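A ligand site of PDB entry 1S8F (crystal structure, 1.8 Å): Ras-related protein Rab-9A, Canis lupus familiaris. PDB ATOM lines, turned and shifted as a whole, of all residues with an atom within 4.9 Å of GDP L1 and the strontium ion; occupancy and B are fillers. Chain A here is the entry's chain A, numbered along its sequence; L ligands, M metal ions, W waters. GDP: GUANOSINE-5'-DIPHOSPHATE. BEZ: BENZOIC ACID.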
ATOM      1  N   ASP A  17      16.951  -3.069 -21.419  1.00  0.00           N
ATOM      2  CA  ASP A  17      16.215  -3.781 -20.390  1.00  0.00           C
ATOM      3  C   ASP A  17      14.752  -4.006 -20.733  1.00  0.00           C
ATOM      4  O   ASP A  17      14.062  -3.294 -21.465  1.00  0.00           O
ATOM      5  CB  ASP A  17      16.272  -3.007 -19.054  1.00  0.00           C
ATOM      6  CG  ASP A  17      17.635  -2.977 -18.413  1.00  0.00           C
ATOM      7  OD1 ASP A  17      18.616  -3.557 -18.931  1.00  0.00           O
ATOM      8  OD2 ASP A  17      17.764  -2.335 -17.334  1.00  0.00           O
ATOM      9  N   GLY A  18      14.211  -5.054 -20.098  1.00  0.00           N
ATOM     10  CA  GLY A  18      12.785  -5.330 -20.237  1.00  0.00           C
ATOM     11  C   GLY A  18      11.982  -4.170 -19.678  1.00  0.00           C
ATOM     12  O   GLY A  18      12.265  -3.601 -18.620  1.00  0.00           O
ATOM     13  N   GLY A  19      10.936  -3.764 -20.383  1.00  0.00           N
ATOM     14  CA  GLY A  19      10.084  -2.694 -19.947  1.00  0.00           C
ATOM     15  C   GLY A  19      10.404  -1.320 -20.470  1.00  0.00           C
ATOM     16  O   GLY A  19       9.575  -0.418 -20.336  1.00  0.00           O
ATOM     17  N   VAL A  20      11.563  -1.091 -21.072  1.00  0.00           N
ATOM     18  CA  VAL A  20      11.913   0.269 -21.493  1.00  0.00           C
ATOM     19  C   VAL A  20      11.101   0.794 -22.676  1.00  0.00           C
ATOM     20  O   VAL A  20      11.078   2.010 -22.922  1.00  0.00           O
ATOM     21  CB  VAL A  20      13.403   0.412 -21.841  1.00  0.00           C
ATOM     22  CG1 VAL A  20      14.293   0.034 -20.666  1.00  0.00           C
ATOM     23  CG2 VAL A  20      13.729  -0.437 -23.070  1.00  0.00           C
ATOM     24  N   GLY A  21      10.433  -0.117 -23.385  1.00  0.00           N
ATOM     25  CA  GLY A  21       9.510   0.205 -24.441  1.00  0.00           C
ATOM     26  C   GLY A  21       9.879  -0.198 -25.841  1.00  0.00           C
ATOM     27  O   GLY A  21       9.382   0.406 -26.791  1.00  0.00           O
ATOM     28  N   LYS A  22      10.690  -1.228 -26.017  1.00  0.00           N
ATOM     29  CA  LYS A  22      11.161  -1.650 -27.352  1.00  0.00           C
ATOM     30  C   LYS A  22      10.015  -2.112 -28.246  1.00  0.00           C
ATOM     31  O   LYS A  22       9.916  -1.641 -29.390  1.00  0.00           O
ATOM     32  CB  LYS A  22      12.209  -2.733 -27.157  1.00  0.00           C
ATOM     33  CG  LYS A  22      13.412  -2.351 -26.319  1.00  0.00           C
ATOM     34  CD  LYS A  22      14.382  -3.519 -26.238  1.00  0.00           C
ATOM     35  CE  LYS A  22      13.803  -4.672 -25.448  1.00  0.00           C
ATOM     36  NZ  LYS A  22      13.466  -4.333 -24.055  1.00  0.00           N
ATOM     37  N   SER A  23       9.173  -3.009 -27.756  1.00  0.00           N
ATOM     38  CA  SER A  23       8.041  -3.554 -28.505  1.00  0.00           C
ATOM     39  C   SER A  23       7.136  -2.407 -28.945  1.00  0.00           C
ATOM     40  O   SER A  23       6.699  -2.284 -30.091  1.00  0.00           O
ATOM     41  CB  SER A  23       7.306  -4.573 -27.658  1.00  0.00           C
ATOM     42  OG  SER A  23       7.943  -5.823 -27.528  1.00  0.00           O
ATOM     43  N   SER A  24       6.864  -1.487 -28.010  1.00  0.00           N
ATOM     44  CA  SER A  24       6.028  -0.339 -28.298  1.00  0.00           C
ATOM     45  C   SER A  24       6.647   0.619 -29.289  1.00  0.00           C
ATOM     46  O   SER A  24       5.911   1.153 -30.132  1.00  0.00           O
ATOM     47  CB  SER A  24       5.736   0.419 -26.991  1.00  0.00           C
ATOM     48  OG  SER A  24       5.168  -0.489 -26.058  1.00  0.00           O
ATOM     49  N   PHE A  34      -0.012   3.109 -30.579  1.00  0.00           N
ATOM     50  CA  PHE A  34       0.430   2.837 -29.225  1.00  0.00           C
ATOM     51  C   PHE A  34      -0.641   1.934 -28.624  1.00  0.00           C
ATOM     52  O   PHE A  34      -1.708   2.375 -28.193  1.00  0.00           O
ATOM     53  CB  PHE A  34       0.661   4.103 -28.402  1.00  0.00           C
ATOM     54  CG  PHE A  34       1.178   3.820 -27.004  1.00  0.00           C
ATOM     55  CD1 PHE A  34       2.467   3.342 -26.811  1.00  0.00           C
ATOM     56  CD2 PHE A  34       0.393   4.029 -25.883  1.00  0.00           C
ATOM     57  CE1 PHE A  34       2.955   3.084 -25.549  1.00  0.00           C
ATOM     58  CE2 PHE A  34       0.877   3.744 -24.626  1.00  0.00           C
ATOM     59  CZ  PHE A  34       2.166   3.266 -24.432  1.00  0.00           C
ATOM     60  N   ASP A  35      -0.371   0.637 -28.638  1.00  0.00           N
ATOM     61  CA  ASP A  35      -1.302  -0.215 -27.911  1.00  0.00           C
ATOM     62  C   ASP A  35      -0.603  -0.677 -26.638  1.00  0.00           C
ATOM     63  O   ASP A  35       0.608  -0.848 -26.713  1.00  0.00           O
ATOM     64  CB  ASP A  35      -1.803  -1.388 -28.757  1.00  0.00           C
ATOM     65  CG  ASP A  35      -3.214  -1.028 -29.231  1.00  0.00           C
ATOM     66  OD1 ASP A  35      -4.103  -0.960 -28.355  1.00  0.00           O
ATOM     67  OD2 ASP A  35      -3.370  -0.833 -30.451  1.00  0.00           O
ATOM     68  N   THR A  36      -1.403  -0.807 -25.603  1.00  0.00           N
ATOM     69  CA  THR A  36      -1.102  -1.095 -24.219  1.00  0.00           C
ATOM     70  C   THR A  36      -1.060  -2.574 -23.881  1.00  0.00           C
ATOM     71  O   THR A  36      -0.618  -2.943 -22.793  1.00  0.00           O
ATOM     72  CB  THR A  36      -2.155  -0.443 -23.284  1.00  0.00           C
ATOM     73  OG1 THR A  36      -1.844  -0.781 -21.920  1.00  0.00           O
ATOM     74  CG2 THR A  36      -3.558  -0.976 -23.519  1.00  0.00           C
ATOM     75  N   LEU A  38       0.618  -5.428 -25.576  1.00  0.00           N
ATOM     76  CA  LEU A  38       1.397  -6.155 -26.581  1.00  0.00           C
ATOM     77  C   LEU A  38       1.720  -7.522 -25.995  1.00  0.00           C
ATOM     78  O   LEU A  38       1.792  -7.647 -24.767  1.00  0.00           O
ATOM     79  CB  LEU A  38       2.656  -5.390 -27.000  1.00  0.00           C
ATOM     80  CG  LEU A  38       2.407  -4.115 -27.821  1.00  0.00           C
ATOM     81  CD1 LEU A  38       3.680  -3.268 -27.891  1.00  0.00           C
ATOM     82  CD2 LEU A  38       1.891  -4.457 -29.209  1.00  0.00           C
ATOM     83  N   PHE A  39       1.905  -8.500 -26.880  1.00  0.00           N
ATOM     84  CA  PHE A  39       2.319  -9.800 -26.366  1.00  0.00           C
ATOM     85  C   PHE A  39       3.680  -9.662 -25.673  1.00  0.00           C
ATOM     86  O   PHE A  39       4.488  -8.831 -26.077  1.00  0.00           O
ATOM     87  CB  PHE A  39       2.451 -10.815 -27.475  1.00  0.00           C
ATOM     88  CG  PHE A  39       1.192 -11.374 -28.085  1.00  0.00           C
ATOM     89  CD1 PHE A  39       0.470 -10.603 -28.976  1.00  0.00           C
ATOM     90  CD2 PHE A  39       0.750 -12.656 -27.787  1.00  0.00           C
ATOM     91  CE1 PHE A  39      -0.673 -11.104 -29.571  1.00  0.00           C
ATOM     92  CE2 PHE A  39      -0.386 -13.164 -28.393  1.00  0.00           C
ATOM     93  CZ  PHE A  39      -1.087 -12.382 -29.287  1.00  0.00           C
ATOM     94  N   GLU A  45      11.305 -10.903 -31.581  1.00  0.00           N
ATOM     95  CA  GLU A  45      10.146 -10.442 -32.332  1.00  0.00           C
ATOM     96  C   GLU A  45      10.642  -9.577 -33.478  1.00  0.00           C
ATOM     97  O   GLU A  45      11.683  -8.942 -33.329  1.00  0.00           O
ATOM     98  CB  GLU A  45       9.208  -9.543 -31.531  1.00  0.00           C
ATOM     99  CG  GLU A  45       9.216  -9.691 -30.027  1.00  0.00           C
ATOM    100  CD  GLU A  45       8.338  -8.695 -29.307  1.00  0.00           C
ATOM    101  OE1 GLU A  45       7.288  -9.100 -28.763  1.00  0.00           O
ATOM    102  OE2 GLU A  45       8.745  -7.524 -29.303  1.00  0.00           O
ATOM    103  N   ASP A  64      13.492  -6.978 -31.877  1.00  0.00           N
ATOM    104  CA  ASP A  64      13.867  -6.701 -30.477  1.00  0.00           C
ATOM    105  C   ASP A  64      13.789  -8.025 -29.737  1.00  0.00           C
ATOM    106  O   ASP A  64      13.569  -9.087 -30.334  1.00  0.00           O
ATOM    107  CB  ASP A  64      13.014  -5.629 -29.808  1.00  0.00           C
ATOM    108  CG  ASP A  64      11.708  -6.134 -29.234  1.00  0.00           C
ATOM    109  OD1 ASP A  64      11.361  -5.701 -28.112  1.00  0.00           O
ATOM    110  OD2 ASP A  64      11.040  -6.949 -29.908  1.00  0.00           O
ATOM    111  N   ASN A 126      13.660   6.466 -23.915  1.00  0.00           N
ATOM    112  CA  ASN A 126      12.232   6.399 -24.140  1.00  0.00           C
ATOM    113  C   ASN A 126      11.424   6.867 -22.923  1.00  0.00           C
ATOM    114  O   ASN A 126      12.003   7.088 -21.862  1.00  0.00           O
ATOM    115  CB  ASN A 126      11.834   4.991 -24.598  1.00  0.00           C
ATOM    116  CG  ASN A 126      10.436   4.875 -25.148  1.00  0.00           C
ATOM    117  OD1 ASN A 126       9.984   5.683 -25.966  1.00  0.00           O
ATOM    118  ND2 ASN A 126       9.686   3.884 -24.665  1.00  0.00           N
ATOM    119  N   LYS A 127      10.135   7.051 -23.138  1.00  0.00           N
ATOM    120  CA  LYS A 127       9.110   7.403 -22.166  1.00  0.00           C
ATOM    121  C   LYS A 127       9.323   8.836 -21.665  1.00  0.00           C
ATOM    122  O   LYS A 127       9.036   9.121 -20.499  1.00  0.00           O
ATOM    123  CB  LYS A 127       9.094   6.431 -20.992  1.00  0.00           C
ATOM    124  CG  LYS A 127       9.067   4.966 -21.388  1.00  0.00           C
ATOM    125  CD  LYS A 127       8.521   4.131 -20.244  1.00  0.00           C
ATOM    126  CE  LYS A 127       8.644   2.639 -20.486  1.00  0.00           C
ATOM    127  NZ  LYS A 127       8.114   1.871 -19.318  1.00  0.00           N
ATOM    128  N   ASP A 129       7.583  11.242 -22.266  1.00  0.00           N
ATOM    129  CA  ASP A 129       6.260  11.689 -21.880  1.00  0.00           C
ATOM    130  C   ASP A 129       6.051  11.618 -20.358  1.00  0.00           C
ATOM    131  O   ASP A 129       5.129  12.222 -19.830  1.00  0.00           O
ATOM    132  CB  ASP A 129       5.157  10.884 -22.569  1.00  0.00           C
ATOM    133  CG  ASP A 129       5.244   9.403 -22.222  1.00  0.00           C
ATOM    134  OD1 ASP A 129       4.562   8.975 -21.265  1.00  0.00           O
ATOM    135  OD2 ASP A 129       6.006   8.713 -22.923  1.00  0.00           O
ATOM    136  N   ILE A 130       6.902  10.868 -19.703  1.00  0.00           N
ATOM    137  CA  ILE A 130       6.951  10.685 -18.256  1.00  0.00           C
ATOM    138  C   ILE A 130       7.744  11.822 -17.643  1.00  0.00           C
ATOM    139  O   ILE A 130       8.969  11.868 -17.724  1.00  0.00           O
ATOM    140  CB  ILE A 130       7.551   9.302 -17.924  1.00  0.00           C
ATOM    141  CG1 ILE A 130       6.727   8.163 -18.536  1.00  0.00           C
ATOM    142  CG2 ILE A 130       7.739   9.111 -16.436  1.00  0.00           C
ATOM    143  CD1 ILE A 130       6.820   6.819 -17.849  1.00  0.00           C
ATOM    144  N   THR A 155      12.658   9.768 -26.858  1.00  0.00           N
ATOM    145  CA  THR A 155      11.478   9.341 -27.570  1.00  0.00           C
ATOM    146  C   THR A 155      10.333   9.044 -26.626  1.00  0.00           C
ATOM    147  O   THR A 155      10.550   8.829 -25.442  1.00  0.00           O
ATOM    148  CB  THR A 155      11.704   8.047 -28.372  1.00  0.00           C
ATOM    149  OG1 THR A 155      12.164   6.997 -27.500  1.00  0.00           O
ATOM    150  CG2 THR A 155      12.811   8.183 -29.405  1.00  0.00           C
ATOM    151  N   SER A 156       9.136   8.991 -27.199  1.00  0.00           N
ATOM    152  CA  SER A 156       7.965   8.470 -26.524  1.00  0.00           C
ATOM    153  C   SER A 156       7.167   7.665 -27.556  1.00  0.00           C
ATOM    154  O   SER A 156       6.618   8.239 -28.490  1.00  0.00           O
ATOM    155  CB  SER A 156       7.090   9.529 -25.889  1.00  0.00           C
ATOM    156  OG  SER A 156       5.864   9.015 -25.392  1.00  0.00           O
ATOM    157  N   ALA A 157       7.145   6.355 -27.353  1.00  0.00           N
ATOM    158  CA  ALA A 157       6.328   5.435 -28.126  1.00  0.00           C
ATOM    159  C   ALA A 157       4.854   5.774 -27.912  1.00  0.00           C
ATOM    160  O   ALA A 157       3.995   5.724 -28.791  1.00  0.00           O
ATOM    161  CB  ALA A 157       6.655   4.012 -27.709  1.00  0.00           C
ATOM    162  N   LYS A 158       4.540   6.169 -26.672  1.00  0.00           N
ATOM    163  CA  LYS A 158       3.171   6.529 -26.334  1.00  0.00           C
ATOM    164  C   LYS A 158       2.671   7.740 -27.125  1.00  0.00           C
ATOM    165  O   LYS A 158       1.558   7.731 -27.646  1.00  0.00           O
ATOM    166  CB  LYS A 158       3.053   6.838 -24.837  1.00  0.00           C
ATOM    167  CG  LYS A 158       1.646   7.261 -24.439  1.00  0.00           C
ATOM    168  CD  LYS A 158       1.554   7.476 -22.924  1.00  0.00           C
ATOM    169  CE  LYS A 158       0.273   8.239 -22.561  1.00  0.00           C
ATOM    170  NZ  LYS A 158       0.310   9.641 -23.056  1.00  0.00           N
HETATM  171  PB  GDP L   1       9.899  -3.682 -23.813  1.00  0.00           P
HETATM  172  O1B GDP L   1      11.158  -2.975 -23.802  1.00  0.00           O
HETATM  173  O2B GDP L   1       9.810  -4.777 -22.792  1.00  0.00           O
HETATM  174  O3B GDP L   1       9.436  -4.344 -25.108  1.00  0.00           O
HETATM  175  O3A GDP L   1       8.789  -2.522 -23.391  1.00  0.00           O
HETATM  176  PA  GDP L   1       7.247  -2.626 -23.867  1.00  0.00           P
HETATM  177  O1A GDP L   1       6.823  -4.056 -23.858  1.00  0.00           O
HETATM  178  O2A GDP L   1       6.973  -2.048 -25.276  1.00  0.00           O
HETATM  179  O5' GDP L   1       6.557  -1.686 -22.793  1.00  0.00           O
HETATM  180  C5' GDP L   1       6.722  -1.878 -21.410  1.00  0.00           C
HETATM  181  C4' GDP L   1       5.646  -0.957 -20.790  1.00  0.00           C
HETATM  182  O4' GDP L   1       6.002   0.383 -21.082  1.00  0.00           O
HETATM  183  C3' GDP L   1       4.298  -1.206 -21.433  1.00  0.00           C
HETATM  184  O3' GDP L   1       3.304  -1.118 -20.426  1.00  0.00           O
HETATM  185  C2' GDP L   1       4.112  -0.056 -22.409  1.00  0.00           C
HETATM  186  O2' GDP L   1       2.806   0.317 -22.754  1.00  0.00           O
HETATM  187  C1' GDP L   1       4.946   1.035 -21.780  1.00  0.00           C
HETATM  188  N9  GDP L   1       5.469   1.974 -22.770  1.00  0.00           N
HETATM  189  C8  GDP L   1       6.229   1.709 -23.880  1.00  0.00           C
HETATM  190  N7  GDP L   1       6.715   2.859 -24.360  1.00  0.00           N
HETATM  191  C5  GDP L   1       6.281   3.888 -23.581  1.00  0.00           C
HETATM  192  C6  GDP L   1       6.451   5.279 -23.578  1.00  0.00           C
HETATM  193  O6  GDP L   1       7.108   5.915 -24.389  1.00  0.00           O
HETATM  194  N1  GDP L   1       5.837   6.032 -22.592  1.00  0.00           N
HETATM  195  C2  GDP L   1       5.060   5.433 -21.604  1.00  0.00           C
HETATM  196  N2  GDP L   1       4.475   6.164 -20.654  1.00  0.00           N
HETATM  197  N3  GDP L   1       4.880   4.069 -21.584  1.00  0.00           N
HETATM  198  C4  GDP L   1       5.494   3.317 -22.570  1.00  0.00           C
HETATM  199  C   BEZ L   2       8.260  -8.425 -22.691  1.00  0.00           C
HETATM  200  O1  BEZ L   2       7.149  -7.598 -22.754  1.00  0.00           O
HETATM  201  O2  BEZ L   2       9.296  -8.080 -23.392  1.00  0.00           O
HETATM  202  C1  BEZ L   2       8.260  -9.663 -21.836  1.00  0.00           C
HETATM  203  C2  BEZ L   2       8.960 -10.781 -22.268  1.00  0.00           C
HETATM  204  C3  BEZ L   2       8.915 -11.884 -21.441  1.00  0.00           C
HETATM  205  C4  BEZ L   2       8.201 -11.868 -20.221  1.00  0.00           C
HETATM  206  C5  BEZ L   2       7.513 -10.755 -19.816  1.00  0.00           C
HETATM  207  C6  BEZ L   2       7.551  -9.645 -20.633  1.00  0.00           C
HETATM  208 SR    SR M   1       8.110  -6.293 -24.883  1.00  0.00          SR
HETATM  209  O   HOH W   1      12.125  -6.667 -23.662  1.00  0.00           O
HETATM  210  O   HOH W   2       1.565   1.960 -20.437  1.00  0.00           O
HETATM  211  O   HOH W   3       5.769  -6.410 -25.005  1.00  0.00           O
HETATM  212  O   HOH W   4       8.205  -5.454 -20.743  1.00  0.00           O
HETATM  213  O   HOH W   5       5.698   2.783 -18.727  1.00  0.00           O
HETATM  214  O   HOH W   6      10.335  -7.110 -25.985  1.00  0.00           O
HETATM  215  O   HOH W   7       4.527  -4.848 -22.966  1.00  0.00           O
HETATM  216  O   HOH W   8       7.521  -8.669 -26.018  1.00  0.00           O
HETATM  217  O   HOH W   9       3.087   5.417 -18.186  1.00  0.00           O
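The backbone NH of Lys 158 sits at hydrogen-bond distance from an oxygen (O6) of GDP L1 (3.4 Å). An oxygen (O2A) of GDP L1 lies within hydrogen-bond range of the side-chain hydroxyl of Ser 24, at 2.5 Å. NZ of Lys 127 is in hydrogen-bond range of O4' of GDP L1, 3.1 Å away. OG of Ser 156 sits close to O6 of GDP L1 (3.5 Å). The side-chain carboxylate (OD2) of Asp 129 sits at hydrogen-bond distance from a nitrogen (N1) of GDP L1 (2.7 Å). An oxygen (O2A) of GDP L1 sits at hydrogen-bond distance from the backbone NH (N) of Ser 23. The side-chain amino group of Lys 22 is in salt-bridge range of an oxygen (O1B) of GDP L1 (2.7 Å). The backbone NH (N) of Gly 19 sits close to an oxygen (O2B) of GDP L1 (2.8 Å). The backbone NH (N) of Lys 22 sits at hydrogen-bond distance from an oxygen (O1B) of GDP L1 (2.9 Å). ND2 of Asn 126 sits at hydrogen-bond distance from N7 of GDP L1. O1B of GDP L1 lies within hydrogen-bond range of N of Val 20. O6 of GDP L1 sits close to N of Lys 127, at 3.5 Å. An oxygen (O3A) of GDP L1 sits at hydrogen-bond distance from the backbone NH (N) of Gly 21 (2.9 Å). O6 of GDP L1 sits at hydrogen-bond distance from N of Ala 157 (3.0 Å). The backbone NH of Ser 24 is in hydrogen-bond range of an oxygen (O2A) of GDP L1 (2.8 Å).
OD1 of Asp 64 is in hydrogen-bond range of N of Ser 23, at 3.5 Å. OG of Ser 156 is in hydrogen-bond range of OD2 of Asp 129 (2.5 Å). The backbone NH (N) of Ala 157 is in hydrogen-bond range of the side-chain amide oxygen (OD1) of Asn 126, at 3.2 Å. The side-chain amide nitrogen (ND2) of Asn 126 lies within hydrogen-bond range of the backbone carbonyl oxygen (O) of Val 20 (2.9 Å). N of Asp 64 sits at hydrogen-bond distance from O of Glu 45 (3.0 Å). The side-chain amide oxygen of Asn 126 sits at hydrogen-bond distance from the side-chain hydroxyl of Thr 155. The side-chain amino group (NZ) of Lys 22 is in hydrogen-bond range of the backbone carbonyl oxygen (O) of Asp 17 (2.9 Å). The backbone NH of Lys 127 sits at hydrogen-bond distance from the backbone carbonyl oxygen of Thr 155 (2.9 Å).
The strontium ion is bound by water W3 (2.3 Å), O3B of GDP L1 (2.4 Å), O2 of BEZ L2 (2.6 Å), water W6 (2.6 Å), O1 of BEZ L2 (2.7 Å), OG of Ser 23 (2.7 Å), water W8 (2.7 Å), O1A of GDP L1 (2.8 Å) and O2B of GDP L1 (3.1 Å). The strontium ion has nine donor atoms within binding distance.
Residues that only touch GDP L1: Asp 17 (3.7 Å), Gly 18 (3.8 Å), Phe 34 (3.5 Å), Asp 64 (3.8 Å) and Ile 130 (3.7 Å). Hydrophobic or aromatic side chains that line GDP L1: Val 20, Phe 34, Ile 130 and Ala 157. Within 4 Å of GDP L1: Asp 17, Gly 18, Gly 19, Val 20, Gly 21, Lys 22, Ser 23, Ser 24, Phe 34, Asp 64, Asn 126, Lys 127, Asp 129, Ile 130, Ser 156, Ala 157 and Lys 158. Along chain A the residues within 4 Å of GDP L1 span positions 17 to 158. The nearest printed residue that does not touch GDP L1 is Leu 38 (4.4 Å).
Within 4 Å of the strontium ion: Ser 23. The nearest printed residue that does not touch the strontium ion is Phe 39 (4.6 Å).
Water W8 lies within hydrogen-bond range of the side-chain carboxylate (OE1) of Glu 45 (2.8 Å) and the backbone carbonyl oxygen (O) of Phe 39 (3.0 Å). Water W5 lies within hydrogen-bond range of NZ of Lys 127 and N3 of GDP L1.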
